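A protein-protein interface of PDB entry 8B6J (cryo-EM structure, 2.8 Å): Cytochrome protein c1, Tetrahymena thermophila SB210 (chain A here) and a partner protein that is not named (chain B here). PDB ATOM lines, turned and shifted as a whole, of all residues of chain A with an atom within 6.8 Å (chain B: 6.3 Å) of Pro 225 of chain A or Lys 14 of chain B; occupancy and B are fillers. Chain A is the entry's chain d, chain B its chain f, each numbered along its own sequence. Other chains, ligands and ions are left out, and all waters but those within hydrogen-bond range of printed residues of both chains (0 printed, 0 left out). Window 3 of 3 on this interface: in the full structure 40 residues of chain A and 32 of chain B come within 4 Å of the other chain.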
ATOM      1  N   ARG A  72      14.870 -24.115  -2.805  1.00  0.00           N
ATOM      2  CA  ARG A  72      13.887 -24.046  -3.879  1.00  0.00           C
ATOM      3  C   ARG A  72      13.517 -25.436  -4.378  1.00  0.00           C
ATOM      4  O   ARG A  72      12.360 -25.691  -4.731  1.00  0.00           O
ATOM      5  CB  ARG A  72      14.427 -23.190  -5.023  1.00  0.00           C
ATOM      6  CG  ARG A  72      14.517 -21.712  -4.692  1.00  0.00           C
ATOM      7  CD  ARG A  72      14.935 -20.894  -5.901  1.00  0.00           C
ATOM      8  NE  ARG A  72      16.304 -21.178  -6.312  1.00  0.00           N
ATOM      9  CZ  ARG A  72      17.377 -20.573  -5.822  1.00  0.00           C
ATOM     10  NH1 ARG A  72      17.282 -19.648  -4.881  1.00  0.00           N
ATOM     11  NH2 ARG A  72      18.577 -20.904  -6.287  1.00  0.00           N
ATOM     12  N   VAL A 218       5.202 -22.828  -9.658  1.00  0.00           N
ATOM     13  CA  VAL A 218       5.549 -22.695  -8.249  1.00  0.00           C
ATOM     14  C   VAL A 218       5.977 -21.259  -7.988  1.00  0.00           C
ATOM     15  O   VAL A 218       6.803 -20.709  -8.725  1.00  0.00           O
ATOM     16  CB  VAL A 218       6.666 -23.675  -7.847  1.00  0.00           C
ATOM     17  CG1 VAL A 218       7.144 -23.388  -6.433  1.00  0.00           C
ATOM     18  CG2 VAL A 218       6.178 -25.110  -7.965  1.00  0.00           C
ATOM     19  N   TYR A 220       8.064 -19.150  -5.640  1.00  0.00           N
ATOM     20  CA  TYR A 220       9.115 -19.341  -4.656  1.00  0.00           C
ATOM     21  C   TYR A 220       8.960 -18.365  -3.494  1.00  0.00           C
ATOM     22  O   TYR A 220       8.364 -17.291  -3.619  1.00  0.00           O
ATOM     23  CB  TYR A 220      10.490 -19.163  -5.295  1.00  0.00           C
ATOM     24  CG  TYR A 220      10.879 -20.271  -6.242  1.00  0.00           C
ATOM     25  CD1 TYR A 220      11.009 -21.577  -5.797  1.00  0.00           C
ATOM     26  CD2 TYR A 220      11.137 -20.009  -7.579  1.00  0.00           C
ATOM     27  CE1 TYR A 220      11.369 -22.589  -6.657  1.00  0.00           C
ATOM     28  CE2 TYR A 220      11.500 -21.016  -8.446  1.00  0.00           C
ATOM     29  CZ  TYR A 220      11.617 -22.302  -7.979  1.00  0.00           C
ATOM     30  OH  TYR A 220      11.979 -23.312  -8.837  1.00  0.00           O
ATOM     31  N   ASP A 222      11.591 -16.972  -2.047  1.00  0.00           N
ATOM     32  CA  ASP A 222      12.643 -15.977  -2.192  1.00  0.00           C
ATOM     33  C   ASP A 222      12.429 -15.054  -3.383  1.00  0.00           C
ATOM     34  O   ASP A 222      13.282 -14.204  -3.649  1.00  0.00           O
ATOM     35  CB  ASP A 222      14.006 -16.665  -2.321  1.00  0.00           C
ATOM     36  CG  ASP A 222      14.103 -17.546  -3.548  1.00  0.00           C
ATOM     37  OD1 ASP A 222      13.099 -17.666  -4.280  1.00  0.00           O
ATOM     38  OD2 ASP A 222      15.186 -18.120  -3.783  1.00  0.00           O
ATOM     39  N   GLY A 223      11.323 -15.204  -4.108  1.00  0.00           N
ATOM     40  CA  GLY A 223      11.040 -14.339  -5.234  1.00  0.00           C
ATOM     41  C   GLY A 223      11.751 -14.701  -6.514  1.00  0.00           C
ATOM     42  O   GLY A 223      11.647 -13.953  -7.492  1.00  0.00           O
ATOM     43  N   THR A 224      12.471 -15.816  -6.544  1.00  0.00           N
ATOM     44  CA  THR A 224      13.177 -16.205  -7.753  1.00  0.00           C
ATOM     45  C   THR A 224      12.177 -16.423  -8.887  1.00  0.00           C
ATOM     46  O   THR A 224      11.086 -16.957  -8.655  1.00  0.00           O
ATOM     47  CB  THR A 224      13.983 -17.482  -7.514  1.00  0.00           C
ATOM     48  OG1 THR A 224      14.874 -17.288  -6.410  1.00  0.00           O
ATOM     49  CG2 THR A 224      14.789 -17.853  -8.749  1.00  0.00           C
ATOM     50  N   PRO A 225      12.500 -16.018 -10.115  1.00  0.00           N
ATOM     51  CA  PRO A 225      11.583 -16.282 -11.229  1.00  0.00           C
ATOM     52  C   PRO A 225      11.317 -17.772 -11.381  1.00  0.00           C
ATOM     53  O   PRO A 225      12.221 -18.601 -11.248  1.00  0.00           O
ATOM     54  CB  PRO A 225      12.323 -15.711 -12.443  1.00  0.00           C
ATOM     55  CG  PRO A 225      13.246 -14.696 -11.880  1.00  0.00           C
ATOM     56  CD  PRO A 225      13.661 -15.219 -10.541  1.00  0.00           C
ATOM     57  N   ALA A 226      10.063 -18.106 -11.667  1.00  0.00           N
ATOM     58  CA  ALA A 226       9.614 -19.493 -11.744  1.00  0.00           C
ATOM     59  C   ALA A 226       9.452 -19.868 -13.213  1.00  0.00           C
ATOM     60  O   ALA A 226       8.418 -19.593 -13.827  1.00  0.00           O
ATOM     61  CB  ALA A 226       8.313 -19.680 -10.973  1.00  0.00           C
ATOM     62  N   SER A 227      10.480 -20.499 -13.772  1.00  0.00           N
ATOM     63  CA  SER A 227      10.452 -21.015 -15.130  1.00  0.00           C
ATOM     64  C   SER A 227      10.847 -22.483 -15.097  1.00  0.00           C
ATOM     65  O   SER A 227      11.601 -22.914 -14.221  1.00  0.00           O
ATOM     66  CB  SER A 227      11.397 -20.235 -16.048  1.00  0.00           C
ATOM     67  OG  SER A 227      12.728 -20.293 -15.572  1.00  0.00           O
ATOM     68  N   GLN A 230      14.516 -23.345 -14.427  1.00  0.00           N
ATOM     69  CA  GLN A 230      14.929 -23.059 -13.057  1.00  0.00           C
ATOM     70  C   GLN A 230      14.324 -24.058 -12.080  1.00  0.00           C
ATOM     71  O   GLN A 230      14.999 -24.520 -11.154  1.00  0.00           O
ATOM     72  CB  GLN A 230      14.530 -21.633 -12.677  1.00  0.00           C
ATOM     73  CG  GLN A 230      14.992 -21.202 -11.293  1.00  0.00           C
ATOM     74  CD  GLN A 230      16.498 -21.115 -11.183  1.00  0.00           C
ATOM     75  OE1 GLN A 230      17.169 -20.630 -12.093  1.00  0.00           O
ATOM     76  NE2 GLN A 230      17.041 -21.590 -10.070  1.00  0.00           N
ATOM     77  N   MET A 231      13.043 -24.387 -12.259  1.00  0.00           N
ATOM     78  CA  MET A 231      12.412 -25.367 -11.384  1.00  0.00           C
ATOM     79  C   MET A 231      13.074 -26.731 -11.528  1.00  0.00           C
ATOM     80  O   MET A 231      13.314 -27.420 -10.530  1.00  0.00           O
ATOM     81  CB  MET A 231      10.918 -25.456 -11.688  1.00  0.00           C
ATOM     82  CG  MET A 231      10.153 -24.183 -11.363  1.00  0.00           C
ATOM     83  SD  MET A 231       8.369 -24.365 -11.521  1.00  0.00           S
ATOM     84  CE  MET A 231       8.218 -24.694 -13.272  1.00  0.00           C
ATOM     85  N   ASP A 234      16.451 -26.554  -9.657  1.00  0.00           N
ATOM     86  CA  ASP A 234      16.288 -26.621  -8.209  1.00  0.00           C
ATOM     87  C   ASP A 234      15.898 -28.024  -7.765  1.00  0.00           C
ATOM     88  O   ASP A 234      16.426 -28.542  -6.772  1.00  0.00           O
ATOM     89  CB  ASP A 234      15.238 -25.610  -7.753  1.00  0.00           C
ATOM     90  CG  ASP A 234      15.676 -24.176  -7.960  1.00  0.00           C
ATOM     91  OD1 ASP A 234      16.896 -23.911  -7.914  1.00  0.00           O
ATOM     92  OD2 ASP A 234      14.799 -23.311  -8.165  1.00  0.00           O
ATOM     93  N   ILE B   9      19.170 -15.064 -23.045  1.00  0.00           N
ATOM     94  CA  ILE B   9      18.974 -16.336 -22.358  1.00  0.00           C
ATOM     95  C   ILE B   9      18.837 -16.048 -20.872  1.00  0.00           C
ATOM     96  O   ILE B   9      17.805 -16.347 -20.262  1.00  0.00           O
ATOM     97  CB  ILE B   9      20.133 -17.312 -22.629  1.00  0.00           C
ATOM     98  CG1 ILE B   9      20.329 -17.511 -24.134  1.00  0.00           C
ATOM     99  CG2 ILE B   9      19.876 -18.642 -21.942  1.00  0.00           C
ATOM    100  CD1 ILE B   9      19.095 -18.002 -24.862  1.00  0.00           C
ATOM    101  N   GLN B  10      19.876 -15.457 -20.281  1.00  0.00           N
ATOM    102  CA  GLN B  10      19.786 -15.048 -18.886  1.00  0.00           C
ATOM    103  C   GLN B  10      18.715 -13.986 -18.695  1.00  0.00           C
ATOM    104  O   GLN B  10      18.130 -13.883 -17.612  1.00  0.00           O
ATOM    105  CB  GLN B  10      21.141 -14.535 -18.400  1.00  0.00           C
ATOM    106  CG  GLN B  10      21.173 -14.188 -16.924  1.00  0.00           C
ATOM    107  CD  GLN B  10      22.581 -13.973 -16.410  1.00  0.00           C
ATOM    108  OE1 GLN B  10      23.549 -14.067 -17.163  1.00  0.00           O
ATOM    109  NE2 GLN B  10      22.702 -13.687 -15.120  1.00  0.00           N
ATOM    110  N   GLU B  11      18.439 -13.195 -19.732  1.00  0.00           N
ATOM    111  CA  GLU B  11      17.356 -12.221 -19.646  1.00  0.00           C
ATOM    112  C   GLU B  11      16.011 -12.919 -19.491  1.00  0.00           C
ATOM    113  O   GLU B  11      15.181 -12.517 -18.669  1.00  0.00           O
ATOM    114  CB  GLU B  11      17.362 -11.324 -20.884  1.00  0.00           C
ATOM    115  CG  GLU B  11      16.336 -10.203 -20.844  1.00  0.00           C
ATOM    116  CD  GLU B  11      16.545  -9.256 -19.675  1.00  0.00           C
ATOM    117  OE1 GLU B  11      17.648  -9.263 -19.091  1.00  0.00           O
ATOM    118  OE2 GLU B  11      15.602  -8.509 -19.341  1.00  0.00           O
ATOM    119  N   TRP B  12      15.776 -13.970 -20.280  1.00  0.00           N
ATOM    120  CA  TRP B  12      14.541 -14.736 -20.137  1.00  0.00           C
ATOM    121  C   TRP B  12      14.496 -15.470 -18.805  1.00  0.00           C
ATOM    122  O   TRP B  12      13.444 -15.530 -18.158  1.00  0.00           O
ATOM    123  CB  TRP B  12      14.393 -15.721 -21.296  1.00  0.00           C
ATOM    124  CG  TRP B  12      13.692 -15.149 -22.492  1.00  0.00           C
ATOM    125  CD1 TRP B  12      13.447 -13.830 -22.750  1.00  0.00           C
ATOM    126  CD2 TRP B  12      13.134 -15.880 -23.590  1.00  0.00           C
ATOM    127  NE1 TRP B  12      12.777 -13.696 -23.939  1.00  0.00           N
ATOM    128  CE2 TRP B  12      12.571 -14.940 -24.475  1.00  0.00           C
ATOM    129  CE3 TRP B  12      13.056 -17.237 -23.910  1.00  0.00           C
ATOM    130  CZ2 TRP B  12      11.941 -15.314 -25.660  1.00  0.00           C
ATOM    131  CZ3 TRP B  12      12.432 -17.607 -25.085  1.00  0.00           C
ATOM    132  CH2 TRP B  12      11.882 -16.649 -25.946  1.00  0.00           C
ATOM    133  N   ILE B  13      15.625 -16.035 -18.376  1.00  0.00           N
ATOM    134  CA  ILE B  13      15.661 -16.732 -17.094  1.00  0.00           C
ATOM    135  C   ILE B  13      15.307 -15.776 -15.964  1.00  0.00           C
ATOM    136  O   ILE B  13      14.599 -16.144 -15.019  1.00  0.00           O
ATOM    137  CB  ILE B  13      17.039 -17.384 -16.883  1.00  0.00           C
ATOM    138  CG1 ILE B  13      17.230 -18.535 -17.875  1.00  0.00           C
ATOM    139  CG2 ILE B  13      17.180 -17.880 -15.451  1.00  0.00           C
ATOM    140  CD1 ILE B  13      18.657 -19.018 -17.994  1.00  0.00           C
ATOM    141  N   LYS B  14      15.792 -14.534 -16.038  1.00  0.00           N
ATOM    142  CA  LYS B  14      15.360 -13.516 -15.089  1.00  0.00           C
ATOM    143  C   LYS B  14      13.857 -13.298 -15.151  1.00  0.00           C
ATOM    144  O   LYS B  14      13.265 -12.830 -14.171  1.00  0.00           O
ATOM    145  CB  LYS B  14      16.094 -12.202 -15.351  1.00  0.00           C
ATOM    146  CG  LYS B  14      17.553 -12.221 -14.938  1.00  0.00           C
ATOM    147  CD  LYS B  14      18.240 -10.905 -15.257  1.00  0.00           C
ATOM    148  CE  LYS B  14      19.693 -10.919 -14.815  1.00  0.00           C
ATOM    149  NZ  LYS B  14      20.384  -9.639 -15.127  1.00  0.00           N
ATOM    150  N   ARG B  15      13.232 -13.611 -16.279  1.00  0.00           N
ATOM    151  CA  ARG B  15      11.787 -13.687 -16.390  1.00  0.00           C
ATOM    152  C   ARG B  15      11.351 -15.138 -16.195  1.00  0.00           C
ATOM    153  O   ARG B  15      12.167 -16.034 -15.969  1.00  0.00           O
ATOM    154  CB  ARG B  15      11.329 -13.134 -17.740  1.00  0.00           C
ATOM    155  CG  ARG B  15      11.636 -11.659 -17.926  1.00  0.00           C
ATOM    156  CD  ARG B  15      12.201 -11.366 -19.305  1.00  0.00           C
ATOM    157  NE  ARG B  15      11.240 -11.627 -20.370  1.00  0.00           N
ATOM    158  CZ  ARG B  15      11.465 -11.392 -21.655  1.00  0.00           C
ATOM    159  NH1 ARG B  15      12.615 -10.890 -22.076  1.00  0.00           N
ATOM    160  NH2 ARG B  15      10.512 -11.665 -22.541  1.00  0.00           N
ATOM    161  N   GLY B  16      10.047 -15.372 -16.278  1.00  0.00           N
ATOM    162  CA  GLY B  16       9.511 -16.704 -16.117  1.00  0.00           C
ATOM    163  C   GLY B  16       9.485 -17.546 -17.369  1.00  0.00           C
ATOM    164  O   GLY B  16       8.998 -18.679 -17.329  1.00  0.00           O
ATOM    165  N   ASN B  79      23.233 -20.229 -16.895  1.00  0.00           N
ATOM    166  CA  ASN B  79      22.606 -18.938 -16.638  1.00  0.00           C
ATOM    167  C   ASN B  79      21.484 -19.016 -15.610  1.00  0.00           C
ATOM    168  O   ASN B  79      20.730 -18.048 -15.460  1.00  0.00           O
ATOM    169  CB  ASN B  79      22.072 -18.349 -17.943  1.00  0.00           C
ATOM    170  CG  ASN B  79      23.176 -18.016 -18.925  1.00  0.00           C
ATOM    171  OD1 ASN B  79      23.621 -16.871 -19.010  1.00  0.00           O
ATOM    172  ND2 ASN B  79      23.628 -19.017 -19.669  1.00  0.00           N
ATOM    173  N   PHE B  81      19.751 -19.331 -11.777  1.00  0.00           N
ATOM    174  CA  PHE B  81      20.016 -18.942 -10.400  1.00  0.00           C
ATOM    175  C   PHE B  81      20.573 -20.126  -9.622  1.00  0.00           C
ATOM    176  O   PHE B  81      20.102 -21.258  -9.760  1.00  0.00           O
ATOM    177  CB  PHE B  81      18.736 -18.439  -9.730  1.00  0.00           C
ATOM    178  CG  PHE B  81      18.163 -17.200 -10.357  1.00  0.00           C
ATOM    179  CD1 PHE B  81      17.363 -17.283 -11.482  1.00  0.00           C
ATOM    180  CD2 PHE B  81      18.412 -15.954  -9.809  1.00  0.00           C
ATOM    181  CE1 PHE B  81      16.831 -16.144 -12.056  1.00  0.00           C
ATOM    182  CE2 PHE B  81      17.881 -14.812 -10.379  1.00  0.00           C
ATOM    183  CZ  PHE B  81      17.089 -14.909 -11.503  1.00  0.00           C
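Of the printed residues of chain B, Arg 72 of chain A touches Phe 81 (3.8 Å).
Tyr 220 of chain A touches none of the printed residues of chain B.
Pro 225 of chain A touches just these residues of chain B: Ile 13, Lys 14, Arg 15 and Phe 81.
Printed residues of chain B within 4 Å of Ala 226 of chain A: Gly 16.
Of the printed residues of chain B, Ser 227 of chain A touches Gly 16.
Of the printed residues of chain B, Gln 230 of chain A touches Phe 81 (2.9 Å).
Asp 234 of chain A touches none of the printed residues of chain B.
Lys 14 of chain B touches just one residue of chain A: Pro 225 (3.0 Å).
Of the printed residues of chain A, Arg 15 of chain B touches Pro 225.
The nearest residue of chain A that does not touch Lys 14 of chain B is Thr 224 of chain A (6.5 Å).
The nearest printed residue of chain A that does not touch Arg 15 of chain B is Ser 227 of chain A (4.3 Å).
The side-chain carboxylate of Asp 222 of chain A is in salt-bridge range of the guanidinium group of Arg 72 of chain A (2.8 Å).
The side-chain carboxylate of Asp 234 of chain A is in salt-bridge range of the guanidinium group of Arg 72 of chain A (3.2 Å).
The side-chain hydroxyl of Thr 224 of chain A sits at hydrogen-bond distance from the side-chain carboxylate of Asp 222 of chain A (2.8 Å).
NE2 of Gln 230 of chain A sits at hydrogen-bond distance from OD1 of Asp 234 of chain A, 3.2 Å away.
Of the 10 printed residues of chain B, 5 touch a printed residue of chain A.
Hydrophobic or aromatic side chains of chain B that line the printed part of chain A: Phe 81.
Of the 12 printed residues of chain A, 6 touch a printed residue of chain B.
Among the printed residues, pairs that only touch across the chains: Pro 225 of chain A with Lys 14 of chain B (3.0 Å), Ser 227 of chain A with Gly 16 of chain B (3.1 Å), Pro 225 of chain A with Ile 13 of chain B (3.5 Å), Pro 225 of chain A with Arg 15 of chain B (3.5 Å), Pro 225 of chain A with Phe 81 of chain B (3.6 Å), Ala 226 of chain A with Gly 16 of chain B (3.7 Å), Thr 224 of chain A with Phe 81 of chain B (3.8 Å) and Arg 72 of chain A with Phe 81 of chain B (3.8 Å).
N of Phe 81 of chain B lies within hydrogen-bond range of OE1 of Gln 230 of chain A (2.9 Å).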
